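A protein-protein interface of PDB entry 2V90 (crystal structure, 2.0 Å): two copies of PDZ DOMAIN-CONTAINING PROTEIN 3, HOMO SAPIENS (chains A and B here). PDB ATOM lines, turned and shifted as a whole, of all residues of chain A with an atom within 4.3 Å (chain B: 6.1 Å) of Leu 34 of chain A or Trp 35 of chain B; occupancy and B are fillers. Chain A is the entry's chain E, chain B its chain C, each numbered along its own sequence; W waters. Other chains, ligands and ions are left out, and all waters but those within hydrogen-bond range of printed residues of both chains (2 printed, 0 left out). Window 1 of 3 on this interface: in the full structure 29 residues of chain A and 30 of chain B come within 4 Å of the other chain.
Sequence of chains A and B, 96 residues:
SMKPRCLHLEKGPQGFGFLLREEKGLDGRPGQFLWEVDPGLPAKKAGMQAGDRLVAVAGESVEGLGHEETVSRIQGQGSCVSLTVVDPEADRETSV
Of chain B, only Trp 35 comes within 4 Å of Leu 34 of chain A.
Of chain A, only Leu 34, Trp 35 and Gly 51 come within 4 Å of Trp 35 of chain B.
Of the printed residues of chain A, Arg 21 of chain B touches Ala 50.
Printed residues of chain B within 4 Å of Gly 51 of chain A: Glu 23 and Trp 35.
Printed residues of chain B within 4 Å of Ala 50 of chain A: Arg 21.
Asp 52 of chain B touches none of the printed residues of chain A.
The nearest residue of chain A that does not touch Trp 35 of chain B is Phe 33 of chain A (4.04 Å).
The nearest printed residue of chain A that does not touch Gly 51 of chain B is Phe 33 of chain A (9.2 Å).
Leu 34 of chain A touches Trp 35 of chain B, but with the chains exchanged Trp 35 of chain A does not touch Leu 34 of chain B (4.01 Å).
Trp 35 of chain B touches its own counterpart, Trp 35 of chain A.
Trp 35 of chain A touches Gly 51 of chain B, and with the chains exchanged Gly 51 of chain A touches Trp 35 of chain B.
Positions printed for both chains: 19, 20, 33, 34, 35, 36, 37, 50, 51 and 52.
Of the 7 pairs that touch across the chains among the printed residues, 3 have their exchanged pair printed and touching as well.
Water W2 bridges the side-chain carboxylate of Glu 36 of chain B and the side-chain carboxylate of Glu 36 of chain A.
Water W1 bridges the side-chain carboxylate (OE1) of Glu 23 of chain B (3.1 Å) and the backbone carbonyl oxygen (O) of Gly 51 of chain A (3.1 Å).
Hydrophobic or aromatic side chains of chain A within 4 Å of the printed part of chain B: Phe 33 and Trp 35.
Along chain A the printed residues that touch a printed residue of chain B span positions 33 to 51.
Along chain B the printed residues that touch a printed residue of chain A span positions 21 to 51.
Among the printed residues, no Asp or Glu carboxylate lies within 4 Å of a Lys or Arg side-chain nitrogen of the other chain.
O of Leu 19 of chain B is in hydrogen-bond range of N of Trp 35 of chain B, at 2.8 Å.
O of Arg 21 of chain B lies within hydrogen-bond range of N of Phe 33 of chain B (2.8 Å).
The backbone NH (N) of Gly 51 of chain B lies within hydrogen-bond range of the backbone carbonyl oxygen (O) of Leu 34 of chain B.
The backbone carbonyl oxygen (O) of Leu 19 of chain A sits at hydrogen-bond distance from the backbone NH (N) of Trp 35 of chain A (2.7 Å).
The backbone carbonyl oxygen (O) of Leu 34 of chain A sits at hydrogen-bond distance from the backbone NH (N) of Gly 51 of chain A, 2.7 Å away.
N of Leu 34 of chain A lies within hydrogen-bond range of O of Asp 52 of chain A, 2.8 Å away.
Among the printed residues, merely in contact across the chains: Phe 33 of chain A with Glu 23 of chain B (3.4 Å), Leu 34 of chain A with Trp 35 of chain B (3.9 Å), Trp 35 of chain A with Gly 51 of chain B (3.9 Å), Ala 50 of chain A with Arg 21 of chain B (3.9 Å) and Gly 51 of chain A with Trp 35 of chain B (3.95 Å).
The side-chain carboxylate (OE2) of Glu 23 of chain B lies close to the backbone carbonyl oxygen (O) of Gly 51 of chain A, at 2.6 Å.
The backbone carbonyl oxygen (O) of Trp 35 of chain B lies within hydrogen-bond range of the indole nitrogen (NE1) of Trp 35 of chain A (2.9 Å).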
ATOM      1  N   PHE A  18      -2.398  10.088 -30.564  1.00  0.00           N
ATOM      2  CA  PHE A  18      -2.008   8.685 -30.587  1.00  0.00           C
ATOM      3  C   PHE A  18      -2.067   8.049 -31.947  1.00  0.00           C
ATOM      4  O   PHE A  18      -2.803   8.488 -32.827  1.00  0.00           O
ATOM      5  CB  PHE A  18      -2.801   7.831 -29.593  1.00  0.00           C
ATOM      6  CG  PHE A  18      -4.261   7.752 -29.877  1.00  0.00           C
ATOM      7  CD1 PHE A  18      -4.771   6.727 -30.681  1.00  0.00           C
ATOM      8  CD2 PHE A  18      -5.148   8.668 -29.296  1.00  0.00           C
ATOM      9  CE1 PHE A  18      -6.144   6.643 -30.921  1.00  0.00           C
ATOM     10  CE2 PHE A  18      -6.505   8.576 -29.529  1.00  0.00           C
ATOM     11  CZ  PHE A  18      -6.997   7.570 -30.347  1.00  0.00           C
ATOM     12  N   LEU A  19      -1.245   7.009 -32.083  1.00  0.00           N
ATOM     13  CA  LEU A  19      -1.150   6.163 -33.263  1.00  0.00           C
ATOM     14  C   LEU A  19      -1.913   4.868 -32.986  1.00  0.00           C
ATOM     15  O   LEU A  19      -1.556   4.116 -32.079  1.00  0.00           O
ATOM     16  CB  LEU A  19       0.324   5.834 -33.554  1.00  0.00           C
ATOM     17  CG  LEU A  19       0.553   4.994 -34.831  1.00  0.00           C
ATOM     18  CD1 LEU A  19       0.183   5.853 -35.987  1.00  0.00           C
ATOM     19  CD2 LEU A  19       1.987   4.565 -34.969  1.00  0.00           C
ATOM     20  N   LEU A  20      -2.946   4.620 -33.790  1.00  0.00           N
ATOM     21  CA  LEU A  20      -3.783   3.448 -33.686  1.00  0.00           C
ATOM     22  C   LEU A  20      -3.321   2.509 -34.763  1.00  0.00           C
ATOM     23  O   LEU A  20      -3.220   2.900 -35.910  1.00  0.00           O
ATOM     24  CB  LEU A  20      -5.260   3.812 -33.946  1.00  0.00           C
ATOM     25  CG  LEU A  20      -6.320   2.783 -33.550  1.00  0.00           C
ATOM     26  CD1 LEU A  20      -6.210   2.424 -32.077  1.00  0.00           C
ATOM     27  CD2 LEU A  20      -7.744   3.318 -33.905  1.00  0.00           C
ATOM     28  N   PHE A  33      -4.720  -1.112 -31.397  1.00  0.00           N
ATOM     29  CA  PHE A  33      -3.852  -0.827 -30.258  1.00  0.00           C
ATOM     30  C   PHE A  33      -3.343   0.571 -30.328  1.00  0.00           C
ATOM     31  O   PHE A  33      -3.093   1.068 -31.426  1.00  0.00           O
ATOM     32  CB  PHE A  33      -2.707  -1.851 -30.193  1.00  0.00           C
ATOM     33  CG  PHE A  33      -3.216  -3.231 -29.980  1.00  0.00           C
ATOM     34  CD1 PHE A  33      -3.474  -3.679 -28.715  1.00  0.00           C
ATOM     35  CD2 PHE A  33      -3.560  -4.027 -31.056  1.00  0.00           C
ATOM     36  CE1 PHE A  33      -4.023  -4.917 -28.489  1.00  0.00           C
ATOM     37  CE2 PHE A  33      -4.112  -5.285 -30.844  1.00  0.00           C
ATOM     38  CZ  PHE A  33      -4.345  -5.724 -29.559  1.00  0.00           C
ATOM     39  N   LEU A  34      -3.181   1.203 -29.163  1.00  0.00           N
ATOM     40  CA  LEU A  34      -2.380   2.433 -29.056  1.00  0.00           C
ATOM     41  C   LEU A  34      -0.900   2.080 -29.186  1.00  0.00           C
ATOM     42  O   LEU A  34      -0.216   1.625 -28.226  1.00  0.00           O
ATOM     43  CB  LEU A  34      -2.674   3.240 -27.781  1.00  0.00           C
ATOM     44  CG  LEU A  34      -4.120   3.635 -27.483  1.00  0.00           C
ATOM     45  CD1 LEU A  34      -4.175   4.795 -26.439  1.00  0.00           C
ATOM     46  CD2 LEU A  34      -4.862   3.994 -28.721  1.00  0.00           C
ATOM     47  N   TRP A  35      -0.415   2.264 -30.410  1.00  0.00           N
ATOM     48  CA  TRP A  35       0.932   1.857 -30.761  1.00  0.00           C
ATOM     49  C   TRP A  35       1.945   2.820 -30.174  1.00  0.00           C
ATOM     50  O   TRP A  35       3.018   2.421 -29.753  1.00  0.00           O
ATOM     51  CB  TRP A  35       1.107   1.786 -32.284  1.00  0.00           C
ATOM     52  CG  TRP A  35       2.112   0.712 -32.720  1.00  0.00           C
ATOM     53  CD1 TRP A  35       3.405   0.899 -33.116  1.00  0.00           C
ATOM     54  CD2 TRP A  35       1.882  -0.709 -32.782  1.00  0.00           C
ATOM     55  NE1 TRP A  35       3.993  -0.311 -33.422  1.00  0.00           N
ATOM     56  CE2 TRP A  35       3.080  -1.311 -33.239  1.00  0.00           C
ATOM     57  CE3 TRP A  35       0.778  -1.525 -32.514  1.00  0.00           C
ATOM     58  CZ2 TRP A  35       3.195  -2.683 -33.429  1.00  0.00           C
ATOM     59  CZ3 TRP A  35       0.896  -2.880 -32.708  1.00  0.00           C
ATOM     60  CH2 TRP A  35       2.093  -3.452 -33.139  1.00  0.00           C
ATOM     61  N   GLU A  36       1.598   4.098 -30.177  1.00  0.00           N
ATOM     62  CA  GLU A  36       2.409   5.157 -29.579  1.00  0.00           C
ATOM     63  C   GLU A  36       1.442   6.228 -29.108  1.00  0.00           C
ATOM     64  O   GLU A  36       0.416   6.459 -29.748  1.00  0.00           O
ATOM     65  CB  GLU A  36       3.365   5.793 -30.606  1.00  0.00           C
ATOM     66  CG  GLU A  36       4.312   4.850 -31.322  1.00  0.00           C
ATOM     67  CD  GLU A  36       5.025   5.497 -32.509  1.00  0.00           C
ATOM     68  OE1 GLU A  36       5.150   6.749 -32.525  1.00  0.00           O
ATOM     69  OE2 GLU A  36       5.469   4.746 -33.422  1.00  0.00           O
ATOM     70  N   VAL A  37       1.769   6.875 -27.993  1.00  0.00           N
ATOM     71  CA  VAL A  37       0.998   7.983 -27.445  1.00  0.00           C
ATOM     72  C   VAL A  37       1.930   9.178 -27.287  1.00  0.00           C
ATOM     73  O   VAL A  37       2.923   9.070 -26.598  1.00  0.00           O
ATOM     74  CB  VAL A  37       0.431   7.625 -26.069  1.00  0.00           C
ATOM     75  CG1 VAL A  37      -0.377   8.794 -25.526  1.00  0.00           C
ATOM     76  CG2 VAL A  37      -0.428   6.350 -26.148  1.00  0.00           C
ATOM     77  N   MET A  48      -3.344   7.615 -20.972  1.00  0.00           N
ATOM     78  CA  MET A  48      -3.271   6.547 -21.986  1.00  0.00           C
ATOM     79  C   MET A  48      -1.816   6.192 -22.258  1.00  0.00           C
ATOM     80  O   MET A  48      -0.945   7.068 -22.263  1.00  0.00           O
ATOM     81  CB  MET A  48      -3.968   6.952 -23.290  1.00  0.00           C
ATOM     82  CG  MET A  48      -5.473   7.120 -23.137  1.00  0.00           C
ATOM     83  SD  MET A  48      -6.320   7.639 -24.660  1.00  0.00           S
ATOM     84  CE  MET A  48      -7.974   7.025 -24.357  1.00  0.00           C
ATOM     85  N   GLN A  49      -1.573   4.901 -22.484  1.00  0.00           N
ATOM     86  CA  GLN A  49      -0.233   4.351 -22.601  1.00  0.00           C
ATOM     87  C   GLN A  49      -0.050   3.617 -23.904  1.00  0.00           C
ATOM     88  O   GLN A  49      -0.982   2.993 -24.374  1.00  0.00           O
ATOM     89  CB  GLN A  49       0.004   3.310 -21.514  1.00  0.00           C
ATOM     90  CG  GLN A  49      -0.523   3.613 -20.139  1.00  0.00           C
ATOM     91  CD  GLN A  49      -0.228   2.466 -19.180  1.00  0.00           C
ATOM     92  OE1 GLN A  49       0.451   1.511 -19.537  1.00  0.00           O
ATOM     93  NE2 GLN A  49      -0.747   2.556 -17.968  1.00  0.00           N
ATOM     94  N   ALA A  50       1.161   3.637 -24.460  1.00  0.00           N
ATOM     95  CA  ALA A  50       1.499   2.705 -25.524  1.00  0.00           C
ATOM     96  C   ALA A  50       1.247   1.254 -25.047  1.00  0.00           C
ATOM     97  O   ALA A  50       1.608   0.893 -23.922  1.00  0.00           O
ATOM     98  CB  ALA A  50       2.929   2.883 -25.956  1.00  0.00           C
ATOM     99  N   GLY A  51       0.631   0.445 -25.904  1.00  0.00           N
ATOM    100  CA  GLY A  51       0.212  -0.918 -25.553  1.00  0.00           C
ATOM    101  C   GLY A  51      -1.211  -1.045 -25.084  1.00  0.00           C
ATOM    102  O   GLY A  51      -1.739  -2.165 -25.004  1.00  0.00           O
ATOM    103  N   ASP A  52      -1.860   0.086 -24.790  1.00  0.00           N
ATOM    104  CA  ASP A  52      -3.299   0.087 -24.510  1.00  0.00           C
ATOM    105  C   ASP A  52      -4.042  -0.505 -25.671  1.00  0.00           C
ATOM    106  O   ASP A  52      -3.713  -0.232 -26.818  1.00  0.00           O
ATOM    107  CB  ASP A  52      -3.835   1.512 -24.340  1.00  0.00           C
ATOM    108  CG  ASP A  52      -3.634   2.050 -22.976  1.00  0.00           C
ATOM    109  OD1 ASP A  52      -3.122   1.316 -22.117  1.00  0.00           O
ATOM    110  OD2 ASP A  52      -3.977   3.214 -22.772  1.00  0.00           O
ATOM    111  N   LEU B  19      11.907  -4.496 -30.458  1.00  0.00           N
ATOM    112  CA  LEU B  19      11.085  -4.465 -29.239  1.00  0.00           C
ATOM    113  C   LEU B  19       9.964  -5.479 -29.415  1.00  0.00           C
ATOM    114  O   LEU B  19       9.184  -5.343 -30.358  1.00  0.00           O
ATOM    115  CB  LEU B  19      10.439  -3.077 -29.097  1.00  0.00           C
ATOM    116  CG  LEU B  19       9.549  -2.835 -27.874  1.00  0.00           C
ATOM    117  CD1 LEU B  19      10.419  -2.932 -26.633  1.00  0.00           C
ATOM    118  CD2 LEU B  19       8.940  -1.457 -27.971  1.00  0.00           C
ATOM    119  N   LEU B  20       9.919  -6.513 -28.590  1.00  0.00           N
ATOM    120  CA  LEU B  20       8.785  -7.466 -28.597  1.00  0.00           C
ATOM    121  C   LEU B  20       7.798  -7.062 -27.511  1.00  0.00           C
ATOM    122  O   LEU B  20       8.203  -6.784 -26.390  1.00  0.00           O
ATOM    123  CB  LEU B  20       9.283  -8.877 -28.349  1.00  0.00           C
ATOM    124  CG  LEU B  20       8.401 -10.071 -28.646  1.00  0.00           C
ATOM    125  CD1 LEU B  20       8.090 -10.176 -30.166  1.00  0.00           C
ATOM    126  CD2 LEU B  20       9.098 -11.320 -28.110  1.00  0.00           C
ATOM    127  N   ARG B  21       6.505  -7.029 -27.838  1.00  0.00           N
ATOM    128  CA  ARG B  21       5.505  -6.722 -26.855  1.00  0.00           C
ATOM    129  C   ARG B  21       4.348  -7.688 -26.961  1.00  0.00           C
ATOM    130  O   ARG B  21       3.901  -8.023 -28.070  1.00  0.00           O
ATOM    131  CB  ARG B  21       4.986  -5.300 -27.018  1.00  0.00           C
ATOM    132  CG  ARG B  21       3.845  -5.027 -26.044  1.00  0.00           C
ATOM    133  CD  ARG B  21       3.155  -3.731 -26.247  1.00  0.00           C
ATOM    134  NE  ARG B  21       3.991  -2.620 -25.846  1.00  0.00           N
ATOM    135  CZ  ARG B  21       4.136  -2.187 -24.601  1.00  0.00           C
ATOM    136  NH1 ARG B  21       3.488  -2.776 -23.581  1.00  0.00           N
ATOM    137  NH2 ARG B  21       4.937  -1.149 -24.384  1.00  0.00           N
ATOM    138  N   GLU B  22       3.904  -8.180 -25.816  1.00  0.00           N
ATOM    139  CA  GLU B  22       2.739  -9.071 -25.776  1.00  0.00           C
ATOM    140  C   GLU B  22       1.423  -8.284 -25.897  1.00  0.00           C
ATOM    141  O   GLU B  22       1.257  -7.241 -25.285  1.00  0.00           O
ATOM    142  CB  GLU B  22       2.748  -9.882 -24.471  1.00  0.00           C
ATOM    143  CG  GLU B  22       1.496 -10.689 -24.252  1.00  0.00           C
ATOM    144  CD  GLU B  22       1.643 -11.650 -23.112  1.00  0.00           C
ATOM    145  OE1 GLU B  22       2.577 -12.463 -23.139  1.00  0.00           O
ATOM    146  OE2 GLU B  22       0.809 -11.602 -22.205  1.00  0.00           O
ATOM    147  N   GLU B  23       0.474  -8.786 -26.675  1.00  0.00           N
ATOM    148  CA  GLU B  23      -0.896  -8.364 -26.523  1.00  0.00           C
ATOM    149  C   GLU B  23      -1.777  -9.567 -26.583  1.00  0.00           C
ATOM    150  O   GLU B  23      -1.709 -10.343 -27.546  1.00  0.00           O
ATOM    151  CB  GLU B  23      -1.328  -7.425 -27.629  1.00  0.00           C
ATOM    152  CG  GLU B  23      -0.685  -6.083 -27.607  1.00  0.00           C
ATOM    153  CD  GLU B  23      -1.144  -5.162 -26.496  1.00  0.00           C
ATOM    154  OE1 GLU B  23      -2.114  -5.490 -25.781  1.00  0.00           O
ATOM    155  OE2 GLU B  23      -0.517  -4.083 -26.357  1.00  0.00           O
ATOM    156  N   PHE B  33       4.327  -9.397 -30.492  1.00  0.00           N
ATOM    157  CA  PHE B  33       4.414  -8.505 -31.643  1.00  0.00           C
ATOM    158  C   PHE B  33       5.736  -7.751 -31.655  1.00  0.00           C
ATOM    159  O   PHE B  33       6.219  -7.344 -30.624  1.00  0.00           O
ATOM    160  CB  PHE B  33       3.252  -7.512 -31.607  1.00  0.00           C
ATOM    161  CG  PHE B  33       1.919  -8.179 -31.700  1.00  0.00           C
ATOM    162  CD1 PHE B  33       1.414  -8.579 -32.933  1.00  0.00           C
ATOM    163  CD2 PHE B  33       1.216  -8.501 -30.546  1.00  0.00           C
ATOM    164  CE1 PHE B  33       0.202  -9.257 -32.997  1.00  0.00           C
ATOM    165  CE2 PHE B  33       0.008  -9.180 -30.630  1.00  0.00           C
ATOM    166  CZ  PHE B  33      -0.473  -9.569 -31.824  1.00  0.00           C
ATOM    167  N   LEU B  34       6.288  -7.556 -32.843  1.00  0.00           N
ATOM    168  CA  LEU B  34       7.493  -6.742 -33.011  1.00  0.00           C
ATOM    169  C   LEU B  34       6.996  -5.295 -33.127  1.00  0.00           C
ATOM    170  O   LEU B  34       6.502  -4.836 -34.168  1.00  0.00           O
ATOM    171  CB  LEU B  34       8.329  -7.244 -34.214  1.00  0.00           C
ATOM    172  CG  LEU B  34       8.588  -8.790 -34.226  1.00  0.00           C
ATOM    173  CD1 LEU B  34       9.048  -9.295 -35.587  1.00  0.00           C
ATOM    174  CD2 LEU B  34       9.578  -9.240 -33.183  1.00  0.00           C
ATOM    175  N   TRP B  35       7.041  -4.621 -31.991  1.00  0.00           N
ATOM    176  CA  TRP B  35       6.436  -3.332 -31.800  1.00  0.00           C
ATOM    177  C   TRP B  35       7.270  -2.239 -32.464  1.00  0.00           C
ATOM    178  O   TRP B  35       6.746  -1.278 -33.008  1.00  0.00           O
ATOM    179  CB  TRP B  35       6.315  -3.061 -30.307  1.00  0.00           C
ATOM    180  CG  TRP B  35       5.102  -2.231 -29.945  1.00  0.00           C
ATOM    181  CD1 TRP B  35       5.049  -0.860 -29.787  1.00  0.00           C
ATOM    182  CD2 TRP B  35       3.771  -2.705 -29.744  1.00  0.00           C
ATOM    183  NE1 TRP B  35       3.772  -0.473 -29.488  1.00  0.00           N
ATOM    184  CE2 TRP B  35       2.960  -1.578 -29.470  1.00  0.00           C
ATOM    185  CE3 TRP B  35       3.180  -3.970 -29.772  1.00  0.00           C
ATOM    186  CZ2 TRP B  35       1.603  -1.688 -29.174  1.00  0.00           C
ATOM    187  CZ3 TRP B  35       1.827  -4.074 -29.508  1.00  0.00           C
ATOM    188  CH2 TRP B  35       1.053  -2.939 -29.209  1.00  0.00           C
ATOM    189  N   GLU B  36       8.584  -2.405 -32.410  1.00  0.00           N
ATOM    190  CA  GLU B  36       9.510  -1.476 -33.044  1.00  0.00           C
ATOM    191  C   GLU B  36      10.674  -2.288 -33.622  1.00  0.00           C
ATOM    192  O   GLU B  36      11.082  -3.292 -33.051  1.00  0.00           O
ATOM    193  CB  GLU B  36      10.006  -0.467 -31.995  1.00  0.00           C
ATOM    194  CG  GLU B  36       8.975   0.579 -31.557  1.00  0.00           C
ATOM    195  CD  GLU B  36       9.306   1.213 -30.203  1.00  0.00           C
ATOM    196  OE1 GLU B  36      10.510   1.287 -29.841  1.00  0.00           O
ATOM    197  OE2 GLU B  36       8.346   1.634 -29.508  1.00  0.00           O
ATOM    198  N   VAL B  37      11.172  -1.889 -34.781  1.00  0.00           N
ATOM    199  CA  VAL B  37      12.361  -2.496 -35.350  1.00  0.00           C
ATOM    200  C   VAL B  37      13.415  -1.389 -35.501  1.00  0.00           C
ATOM    201  O   VAL B  37      13.241  -0.446 -36.251  1.00  0.00           O
ATOM    202  CB  VAL B  37      12.056  -3.235 -36.674  1.00  0.00           C
ATOM    203  CG1 VAL B  37      13.304  -3.898 -37.178  1.00  0.00           C
ATOM    204  CG2 VAL B  37      10.981  -4.296 -36.422  1.00  0.00           C
ATOM    205  N   ALA B  50       8.102  -3.402 -38.165  1.00  0.00           N
ATOM    206  CA  ALA B  50       7.211  -3.119 -37.025  1.00  0.00           C
ATOM    207  C   ALA B  50       5.780  -3.537 -37.424  1.00  0.00           C
ATOM    208  O   ALA B  50       5.331  -3.280 -38.558  1.00  0.00           O
ATOM    209  CB  ALA B  50       7.256  -1.656 -36.602  1.00  0.00           C
ATOM    210  N   GLY B  51       5.097  -4.211 -36.510  1.00  0.00           N
ATOM    211  CA  GLY B  51       3.760  -4.804 -36.799  1.00  0.00           C
ATOM    212  C   GLY B  51       3.791  -6.302 -37.110  1.00  0.00           C
ATOM    213  O   GLY B  51       2.742  -6.977 -37.082  1.00  0.00           O
ATOM    214  N   ASP B  52       4.986  -6.834 -37.396  1.00  0.00           N
ATOM    215  CA  ASP B  52       5.171  -8.277 -37.515  1.00  0.00           C
ATOM    216  C   ASP B  52       4.695  -8.997 -36.260  1.00  0.00           C
ATOM    217  O   ASP B  52       4.870  -8.503 -35.132  1.00  0.00           O
ATOM    218  CB  ASP B  52       6.645  -8.612 -37.751  1.00  0.00           C
ATOM    219  CG  ASP B  52       7.082  -8.451 -39.194  1.00  0.00           C
ATOM    220  OD1 ASP B  52       6.268  -8.069 -40.068  1.00  0.00           O
ATOM    221  OD2 ASP B  52       8.290  -8.700 -39.444  1.00  0.00           O
HETATM  222  O   HOH W   1      -3.671  -4.080 -23.567  1.00  0.00           O
HETATM  223  O   HOH W   2       6.360   2.498 -31.503  1.00  0.00           O
